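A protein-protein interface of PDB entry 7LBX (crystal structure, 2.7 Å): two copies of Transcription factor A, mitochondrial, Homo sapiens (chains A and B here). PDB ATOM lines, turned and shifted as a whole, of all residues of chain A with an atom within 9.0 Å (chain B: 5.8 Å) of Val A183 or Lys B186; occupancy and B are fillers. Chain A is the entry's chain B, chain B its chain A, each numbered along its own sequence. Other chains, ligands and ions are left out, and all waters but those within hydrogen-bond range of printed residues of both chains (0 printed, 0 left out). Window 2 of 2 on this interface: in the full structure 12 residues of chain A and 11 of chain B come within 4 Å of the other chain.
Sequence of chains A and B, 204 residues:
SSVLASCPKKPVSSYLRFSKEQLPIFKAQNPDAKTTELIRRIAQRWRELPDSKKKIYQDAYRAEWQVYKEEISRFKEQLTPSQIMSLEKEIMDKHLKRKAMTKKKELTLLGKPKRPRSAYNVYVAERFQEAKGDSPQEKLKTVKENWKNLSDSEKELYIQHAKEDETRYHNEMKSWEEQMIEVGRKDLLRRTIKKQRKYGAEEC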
ATOM      1  N   GLU A 106      15.254   5.448 -17.209  1.00  0.00           N
ATOM      2  CA  GLU A 106      16.134   4.469 -17.833  1.00  0.00           C
ATOM      3  C   GLU A 106      17.223   4.120 -16.870  1.00  0.00           C
ATOM      4  O   GLU A 106      17.398   2.957 -16.555  1.00  0.00           O
ATOM      5  CB  GLU A 106      16.717   5.078 -19.115  1.00  0.00           C
ATOM      6  CG  GLU A 106      17.693   4.225 -19.900  1.00  0.00           C
ATOM      7  CD  GLU A 106      18.453   5.071 -20.903  1.00  0.00           C
ATOM      8  OE1 GLU A 106      19.291   5.899 -20.473  1.00  0.00           O
ATOM      9  OE2 GLU A 106      18.175   4.941 -22.118  1.00  0.00           O
ATOM     10  N   LEU A 110      17.831   0.528 -15.378  1.00  0.00           N
ATOM     11  CA  LEU A 110      19.135  -0.097 -15.494  1.00  0.00           C
ATOM     12  C   LEU A 110      19.776  -0.355 -14.145  1.00  0.00           C
ATOM     13  O   LEU A 110      20.783  -1.049 -14.087  1.00  0.00           O
ATOM     14  CB  LEU A 110      20.054   0.755 -16.366  1.00  0.00           C
ATOM     15  CG  LEU A 110      19.633   0.899 -17.828  1.00  0.00           C
ATOM     16  CD1 LEU A 110      20.603   1.799 -18.583  1.00  0.00           C
ATOM     17  CD2 LEU A 110      19.510  -0.457 -18.518  1.00  0.00           C
ATOM     18  N   TRP A 176      27.503  -2.165 -11.509  1.00  0.00           N
ATOM     19  CA  TRP A 176      26.548  -1.640 -12.519  1.00  0.00           C
ATOM     20  C   TRP A 176      27.278  -1.294 -13.821  1.00  0.00           C
ATOM     21  O   TRP A 176      26.755  -1.646 -14.888  1.00  0.00           O
ATOM     22  CB  TRP A 176      25.805  -0.427 -11.943  1.00  0.00           C
ATOM     23  CG  TRP A 176      24.947   0.312 -12.923  1.00  0.00           C
ATOM     24  CD1 TRP A 176      23.706  -0.045 -13.359  1.00  0.00           C
ATOM     25  CD2 TRP A 176      25.257   1.553 -13.583  1.00  0.00           C
ATOM     26  NE1 TRP A 176      23.225   0.880 -14.246  1.00  0.00           N
ATOM     27  CE2 TRP A 176      24.155   1.873 -14.403  1.00  0.00           C
ATOM     28  CE3 TRP A 176      26.354   2.421 -13.564  1.00  0.00           C
ATOM     29  CZ2 TRP A 176      24.124   3.017 -15.197  1.00  0.00           C
ATOM     30  CZ3 TRP A 176      26.323   3.553 -14.348  1.00  0.00           C
ATOM     31  CH2 TRP A 176      25.222   3.844 -15.153  1.00  0.00           C
ATOM     32  N   GLU A 177      28.454  -0.668 -13.735  1.00  0.00           N
ATOM     33  CA  GLU A 177      29.159  -0.202 -14.959  1.00  0.00           C
ATOM     34  C   GLU A 177      29.643  -1.398 -15.784  1.00  0.00           C
ATOM     35  O   GLU A 177      29.669  -1.287 -17.021  1.00  0.00           O
ATOM     36  CB  GLU A 177      30.303   0.744 -14.592  1.00  0.00           C
ATOM     37  CG  GLU A 177      29.836   2.152 -14.284  1.00  0.00           C
ATOM     38  CD  GLU A 177      30.880   3.044 -13.635  1.00  0.00           C
ATOM     39  OE1 GLU A 177      31.460   2.627 -12.614  1.00  0.00           O
ATOM     40  OE2 GLU A 177      31.111   4.152 -14.156  1.00  0.00           O
ATOM     41  N   GLU A 178      30.020  -2.493 -15.125  1.00  0.00           N
ATOM     42  CA  GLU A 178      30.423  -3.710 -15.876  1.00  0.00           C
ATOM     43  C   GLU A 178      29.182  -4.289 -16.554  1.00  0.00           C
ATOM     44  O   GLU A 178      29.291  -4.735 -17.711  1.00  0.00           O
ATOM     45  CB  GLU A 178      31.032  -4.743 -14.927  1.00  0.00           C
ATOM     46  CG  GLU A 178      31.941  -4.145 -13.873  1.00  0.00           C
ATOM     47  CD  GLU A 178      32.194  -5.061 -12.689  1.00  0.00           C
ATOM     48  OE1 GLU A 178      33.235  -4.891 -12.023  1.00  0.00           O
ATOM     49  OE2 GLU A 178      31.352  -5.944 -12.437  1.00  0.00           O
ATOM     50  N   GLN A 179      28.048  -4.279 -15.853  1.00  0.00           N
ATOM     51  CA  GLN A 179      26.801  -4.829 -16.401  1.00  0.00           C
ATOM     52  C   GLN A 179      26.283  -3.957 -17.558  1.00  0.00           C
ATOM     53  O   GLN A 179      25.549  -4.461 -18.396  1.00  0.00           O
ATOM     54  CB  GLN A 179      25.718  -5.000 -15.313  1.00  0.00           C
ATOM     55  CG  GLN A 179      25.971  -6.193 -14.374  1.00  0.00           C
ATOM     56  CD  GLN A 179      25.529  -7.587 -14.828  1.00  0.00           C
ATOM     57  OE1 GLN A 179      25.551  -8.529 -14.025  1.00  0.00           O
ATOM     58  NE2 GLN A 179      25.134  -7.808 -16.090  1.00  0.00           N
ATOM     59  N   MET A 180      26.668  -2.659 -17.598  1.00  0.00           N
ATOM     60  CA  MET A 180      26.296  -1.689 -18.633  1.00  0.00           C
ATOM     61  C   MET A 180      27.184  -1.802 -19.871  1.00  0.00           C
ATOM     62  O   MET A 180      26.687  -1.582 -20.985  1.00  0.00           O
ATOM     63  CB  MET A 180      26.326  -0.233 -18.093  1.00  0.00           C
ATOM     64  CG  MET A 180      25.176   0.141 -17.147  1.00  0.00           C
ATOM     65  SD  MET A 180      23.553  -0.614 -17.489  1.00  0.00           S
ATOM     66  CE  MET A 180      23.548  -2.052 -16.414  1.00  0.00           C
ATOM     67  N   ILE A 181      28.475  -2.170 -19.708  1.00  0.00           N
ATOM     68  CA  ILE A 181      29.344  -2.367 -20.875  1.00  0.00           C
ATOM     69  C   ILE A 181      28.867  -3.637 -21.667  1.00  0.00           C
ATOM     70  O   ILE A 181      29.076  -3.697 -22.876  1.00  0.00           O
ATOM     71  CB  ILE A 181      30.861  -2.326 -20.513  1.00  0.00           C
ATOM     72  CG1 ILE A 181      31.699  -1.820 -21.702  1.00  0.00           C
ATOM     73  CG2 ILE A 181      31.385  -3.658 -19.986  1.00  0.00           C
ATOM     74  CD1 ILE A 181      31.530  -0.316 -22.050  1.00  0.00           C
ATOM     75  N   GLU A 182      28.148  -4.585 -20.998  1.00  0.00           N
ATOM     76  CA  GLU A 182      27.467  -5.725 -21.640  1.00  0.00           C
ATOM     77  C   GLU A 182      26.278  -5.215 -22.505  1.00  0.00           C
ATOM     78  O   GLU A 182      26.014  -5.777 -23.566  1.00  0.00           O
ATOM     79  CB  GLU A 182      26.901  -6.699 -20.603  1.00  0.00           C
ATOM     80  CG  GLU A 182      27.922  -7.435 -19.770  1.00  0.00           C
ATOM     81  CD  GLU A 182      27.303  -8.458 -18.836  1.00  0.00           C
ATOM     82  OE1 GLU A 182      26.055  -8.508 -18.733  1.00  0.00           O
ATOM     83  OE2 GLU A 182      28.073  -9.222 -18.211  1.00  0.00           O
ATOM     84  N   VAL A 183      25.532  -4.186 -22.018  1.00  0.00           N
ATOM     85  CA  VAL A 183      24.452  -3.540 -22.781  1.00  0.00           C
ATOM     86  C   VAL A 183      25.151  -2.853 -23.952  1.00  0.00           C
ATOM     87  O   VAL A 183      24.651  -2.899 -25.069  1.00  0.00           O
ATOM     88  CB  VAL A 183      23.603  -2.518 -21.950  1.00  0.00           C
ATOM     89  CG1 VAL A 183      22.512  -1.859 -22.810  1.00  0.00           C
ATOM     90  CG2 VAL A 183      22.984  -3.188 -20.720  1.00  0.00           C
ATOM     91  N   GLY A 184      26.314  -2.256 -23.681  1.00  0.00           N
ATOM     92  CA  GLY A 184      27.150  -1.612 -24.685  1.00  0.00           C
ATOM     93  C   GLY A 184      26.873  -0.136 -24.713  1.00  0.00           C
ATOM     94  O   GLY A 184      26.440   0.404 -25.735  1.00  0.00           O
ATOM     95  N   ARG A 185      27.112   0.514 -23.565  1.00  0.00           N
ATOM     96  CA  ARG A 185      26.815   1.920 -23.404  1.00  0.00           C
ATOM     97  C   ARG A 185      27.899   2.716 -22.699  1.00  0.00           C
ATOM     98  O   ARG A 185      27.790   2.985 -21.516  1.00  0.00           O
ATOM     99  CB  ARG A 185      25.458   2.057 -22.699  1.00  0.00           C
ATOM    100  CG  ARG A 185      24.293   1.869 -23.663  1.00  0.00           C
ATOM    101  CD  ARG A 185      23.077   2.709 -23.327  1.00  0.00           C
ATOM    102  NE  ARG A 185      21.853   1.913 -23.317  1.00  0.00           N
ATOM    103  CZ  ARG A 185      20.625   2.415 -23.237  1.00  0.00           C
ATOM    104  NH1 ARG A 185      20.439   3.731 -23.171  1.00  0.00           N
ATOM    105  NH2 ARG A 185      19.570   1.609 -23.233  1.00  0.00           N
ATOM    106  N   LYS A 186      28.898   3.180 -23.474  1.00  0.00           N
ATOM    107  CA  LYS A 186      29.939   4.109 -23.030  1.00  0.00           C
ATOM    108  C   LYS A 186      29.278   5.475 -22.865  1.00  0.00           C
ATOM    109  O   LYS A 186      29.860   6.328 -22.187  1.00  0.00           O
ATOM    110  CB  LYS A 186      31.108   4.204 -24.055  1.00  0.00           C
ATOM    111  CG  LYS A 186      32.244   5.223 -23.763  1.00  0.00           C
ATOM    112  CD  LYS A 186      32.939   5.036 -22.409  1.00  0.00           C
ATOM    113  CE  LYS A 186      34.002   6.071 -22.101  1.00  0.00           C
ATOM    114  NZ  LYS A 186      35.233   5.898 -22.917  1.00  0.00           N
ATOM    115  N   ASP A 187      28.065   5.697 -23.487  1.00  0.00           N
ATOM    116  CA  ASP A 187      27.345   6.964 -23.321  1.00  0.00           C
ATOM    117  C   ASP A 187      26.968   7.227 -21.853  1.00  0.00           C
ATOM    118  O   ASP A 187      26.936   8.391 -21.443  1.00  0.00           O
ATOM    119  CB  ASP A 187      26.089   7.030 -24.203  1.00  0.00           C
ATOM    120  CG  ASP A 187      25.025   5.996 -23.870  1.00  0.00           C
ATOM    121  OD1 ASP A 187      25.314   4.793 -23.997  1.00  0.00           O
ATOM    122  OD2 ASP A 187      23.885   6.401 -23.525  1.00  0.00           O
ATOM    123  N   LEU A 188      26.684   6.147 -21.071  1.00  0.00           N
ATOM    124  CA  LEU A 188      26.324   6.239 -19.655  1.00  0.00           C
ATOM    125  C   LEU A 188      27.536   6.399 -18.716  1.00  0.00           C
ATOM    126  O   LEU A 188      27.330   6.682 -17.547  1.00  0.00           O
ATOM    127  CB  LEU A 188      25.523   5.000 -19.229  1.00  0.00           C
ATOM    128  CG  LEU A 188      24.229   4.741 -19.986  1.00  0.00           C
ATOM    129  CD1 LEU A 188      23.566   3.468 -19.487  1.00  0.00           C
ATOM    130  CD2 LEU A 188      23.274   5.928 -19.877  1.00  0.00           C
ATOM    131  N   LEU A 189      28.793   6.226 -19.205  1.00  0.00           N
ATOM    132  CA  LEU A 189      30.031   6.361 -18.407  1.00  0.00           C
ATOM    133  C   LEU A 189      30.735   7.678 -18.783  1.00  0.00           C
ATOM    134  O   LEU A 189      30.270   8.383 -19.683  1.00  0.00           O
ATOM    135  CB  LEU A 189      30.983   5.175 -18.710  1.00  0.00           C
ATOM    136  CG  LEU A 189      30.682   3.822 -18.049  1.00  0.00           C
ATOM    137  CD1 LEU A 189      29.494   3.118 -18.678  1.00  0.00           C
ATOM    138  CD2 LEU A 189      31.889   2.896 -18.131  1.00  0.00           C
ATOM    139  N   MET B 180      29.132   1.016 -34.280  1.00  0.00           N
ATOM    140  CA  MET B 180      28.765   1.779 -33.083  1.00  0.00           C
ATOM    141  C   MET B 180      28.405   0.875 -31.911  1.00  0.00           C
ATOM    142  O   MET B 180      28.885   1.147 -30.815  1.00  0.00           O
ATOM    143  CB  MET B 180      27.700   2.810 -33.385  1.00  0.00           C
ATOM    144  CG  MET B 180      28.219   3.916 -34.283  1.00  0.00           C
ATOM    145  SD  MET B 180      29.287   5.087 -33.428  1.00  0.00           S
ATOM    146  CE  MET B 180      30.802   4.827 -34.239  1.00  0.00           C
ATOM    147  N   ILE B 181      27.705  -0.254 -32.130  1.00  0.00           N
ATOM    148  CA  ILE B 181      27.452  -1.203 -31.033  1.00  0.00           C
ATOM    149  C   ILE B 181      28.810  -1.575 -30.371  1.00  0.00           C
ATOM    150  O   ILE B 181      28.974  -1.451 -29.134  1.00  0.00           O
ATOM    151  CB  ILE B 181      26.730  -2.480 -31.540  1.00  0.00           C
ATOM    152  CG1 ILE B 181      25.262  -2.176 -31.880  1.00  0.00           C
ATOM    153  CG2 ILE B 181      26.859  -3.647 -30.525  1.00  0.00           C
ATOM    154  CD1 ILE B 181      24.518  -3.320 -32.417  1.00  0.00           C
ATOM    155  N   GLY B 184      30.616   0.711 -28.101  1.00  0.00           N
ATOM    156  CA  GLY B 184      29.821   0.972 -26.903  1.00  0.00           C
ATOM    157  C   GLY B 184      28.944   2.211 -27.043  1.00  0.00           C
ATOM    158  O   GLY B 184      28.996   3.084 -26.181  1.00  0.00           O
ATOM    159  N   ARG B 185      28.169   2.338 -28.155  1.00  0.00           N
ATOM    160  CA  ARG B 185      27.296   3.489 -28.388  1.00  0.00           C
ATOM    161  C   ARG B 185      25.965   3.047 -29.037  1.00  0.00           C
ATOM    162  O   ARG B 185      25.534   3.623 -30.034  1.00  0.00           O
ATOM    163  CB  ARG B 185      28.020   4.562 -29.220  1.00  0.00           C
ATOM    164  CG  ARG B 185      29.222   5.241 -28.533  1.00  0.00           C
ATOM    165  CD  ARG B 185      28.872   6.065 -27.302  1.00  0.00           C
ATOM    166  NE  ARG B 185      27.824   7.049 -27.584  1.00  0.00           N
ATOM    167  CZ  ARG B 185      28.011   8.294 -28.020  1.00  0.00           C
ATOM    168  NH1 ARG B 185      29.239   8.763 -28.226  1.00  0.00           N
ATOM    169  NH2 ARG B 185      26.968   9.089 -28.237  1.00  0.00           N
ATOM    170  N   LYS B 186      25.293   2.035 -28.430  1.00  0.00           N
ATOM    171  CA  LYS B 186      23.970   1.540 -28.851  1.00  0.00           C
ATOM    172  C   LYS B 186      22.911   2.681 -28.821  1.00  0.00           C
ATOM    173  O   LYS B 186      21.905   2.571 -29.515  1.00  0.00           O
ATOM    174  CB  LYS B 186      23.480   0.386 -27.955  1.00  0.00           C
ATOM    175  CG  LYS B 186      24.296  -0.894 -28.050  1.00  0.00           C
ATOM    176  CD  LYS B 186      23.458  -2.133 -28.435  1.00  0.00           C
ATOM    177  CE  LYS B 186      22.570  -2.686 -27.332  1.00  0.00           C
ATOM    178  NZ  LYS B 186      22.969  -4.070 -26.927  1.00  0.00           N
ATOM    179  N   ASP B 187      23.117   3.743 -27.980  1.00  0.00           N
ATOM    180  CA  ASP B 187      22.261   4.946 -27.891  1.00  0.00           C
ATOM    181  C   ASP B 187      22.097   5.674 -29.256  1.00  0.00           C
ATOM    182  O   ASP B 187      21.080   6.350 -29.466  1.00  0.00           O
ATOM    183  CB  ASP B 187      22.827   5.954 -26.863  1.00  0.00           C
ATOM    184  CG  ASP B 187      24.207   6.472 -27.202  1.00  0.00           C
ATOM    185  OD1 ASP B 187      25.140   5.654 -27.268  1.00  0.00           O
ATOM    186  OD2 ASP B 187      24.361   7.705 -27.369  1.00  0.00           O
ATOM    187  N   LEU B 188      23.105   5.565 -30.145  1.00  0.00           N
ATOM    188  CA  LEU B 188      23.108   6.193 -31.473  1.00  0.00           C
ATOM    189  C   LEU B 188      22.301   5.440 -32.524  1.00  0.00           C
ATOM    190  O   LEU B 188      22.044   6.001 -33.592  1.00  0.00           O
ATOM    191  CB  LEU B 188      24.544   6.340 -31.976  1.00  0.00           C
ATOM    192  CG  LEU B 188      25.481   7.178 -31.111  1.00  0.00           C
ATOM    193  CD1 LEU B 188      26.880   7.156 -31.681  1.00  0.00           C
ATOM    194  CD2 LEU B 188      24.962   8.595 -30.937  1.00  0.00           C
ATOM    195  N   LEU B 189      21.949   4.179 -32.257  1.00  0.00           N
ATOM    196  CA  LEU B 189      21.206   3.340 -33.199  1.00  0.00           C
ATOM    197  C   LEU B 189      19.767   3.790 -33.437  1.00  0.00           C
ATOM    198  O   LEU B 189      19.119   4.301 -32.529  1.00  0.00           O
ATOM    199  CB  LEU B 189      21.208   1.868 -32.741  1.00  0.00           C
ATOM    200  CG  LEU B 189      22.385   1.030 -33.256  1.00  0.00           C
ATOM    201  CD1 LEU B 189      23.716   1.649 -32.896  1.00  0.00           C
ATOM    202  CD2 LEU B 189      22.300  -0.363 -32.752  1.00  0.00           C
ATOM    203  N   ARG B 191      15.992   3.576 -33.369  1.00  0.00           N
ATOM    204  CA  ARG B 191      15.036   2.861 -32.524  1.00  0.00           C
ATOM    205  C   ARG B 191      13.745   2.630 -33.311  1.00  0.00           C
ATOM    206  O   ARG B 191      13.469   1.508 -33.734  1.00  0.00           O
ATOM    207  CB  ARG B 191      14.759   3.671 -31.238  1.00  0.00           C
ATOM    208  CG  ARG B 191      14.662   2.836 -29.950  1.00  0.00           C
ATOM    209  CD  ARG B 191      15.945   2.095 -29.586  1.00  0.00           C
ATOM    210  NE  ARG B 191      17.091   3.001 -29.470  1.00  0.00           N
ATOM    211  CZ  ARG B 191      18.372   2.643 -29.532  1.00  0.00           C
ATOM    212  NH1 ARG B 191      18.710   1.369 -29.727  1.00  0.00           N
ATOM    213  NH2 ARG B 191      19.326   3.554 -29.411  1.00  0.00           N
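The backbone carbonyl oxygen (O) of Gly B184 is in hydrogen-bond range of the backbone NH (N) of Lys A186, at 2.7 Å. The side-chain amino group of Lys B186 is in hydrogen-bond range of the backbone carbonyl oxygen of Val A183 (2.8 Å). The backbone NH (N) of Lys B186 lies within hydrogen-bond range of the backbone carbonyl oxygen (O) of Gly A184. OD1 of Asp A187 lies close to OD1 of Asp B187 (3.4 Å).
N of Arg B185 is in hydrogen-bond range of O of Met B180 (3.0 Å). The side-chain carboxylate (OD1) of Asp B187 is in salt-bridge range of the guanidinium group (NE) of Arg B185 (3.0 Å). The guanidinium group (NH2) of Arg B191 is in hydrogen-bond range of the backbone carbonyl oxygen (O) of Lys B186, 2.8 Å away. The guanidinium group of Arg B191 lies within hydrogen-bond range of the backbone carbonyl oxygen of Asp B187, 3.3 Å away. OE2 of Glu A106 lies within salt-bridge range of NH1 of Arg A185, at 2.8 Å. O of Met A180 lies within hydrogen-bond range of N of Arg A185 (3.4 Å).
Among the printed residues, merely in contact across the chains: Gly A184 with Gly B184 (3.4 Å), Gly A184 with Arg B185 (3.5 Å), Arg A185 with Gly B184 (3.7 Å), Asp A187 with Gly B184 (3.9 Å) and Asp A187 with Arg B185 (3.8 Å).
Trp A176 touches none of the printed residues of chain B. Glu A177 touches none of the printed residues of chain B. Val A183 touches just one residue of chain B: Lys B186. Of the printed residues of chain B, Gly A184 touches Gly B184 (3.4 Å), Arg B185 (3.5 Å) and Lys B186 (3.4 Å). Of the printed residues of chain B, Lys A186 touches Gly B184 (2.7 Å). Of the printed residues of chain A, Arg B185 touches Gly A184 and Asp A187. Lys B186 touches just these residues of chain A: Val A183 and Gly A184. The nearest printed residue of chain B that does not touch Val A183 is Ile B181 (5.9 Å). The nearest printed residue of chain B that does not touch Arg A185 is Lys B186 (4.6 Å).
Of the 9 printed residues of chain B, 4 touch a printed residue of chain A. Of the 16 printed residues of chain A, 5 touch a printed residue of chain B. Among the printed residues, 9 pairs touch across the chains.
Gly A184 touches Arg B185, and with the chains exchanged Arg A185 touches Gly B184. Gly A184 touches Lys B186, and with the chains exchanged Lys A186 touches Gly B184. Asp A187 touches Arg B185, but with the chains exchanged Arg A185 does not touch Asp B187 (4.8 Å). Asp A187 touches its own counterpart, Asp B187. Positions printed for both chains: 180, 181, 184, 185, 186, 187, 188 and 189.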
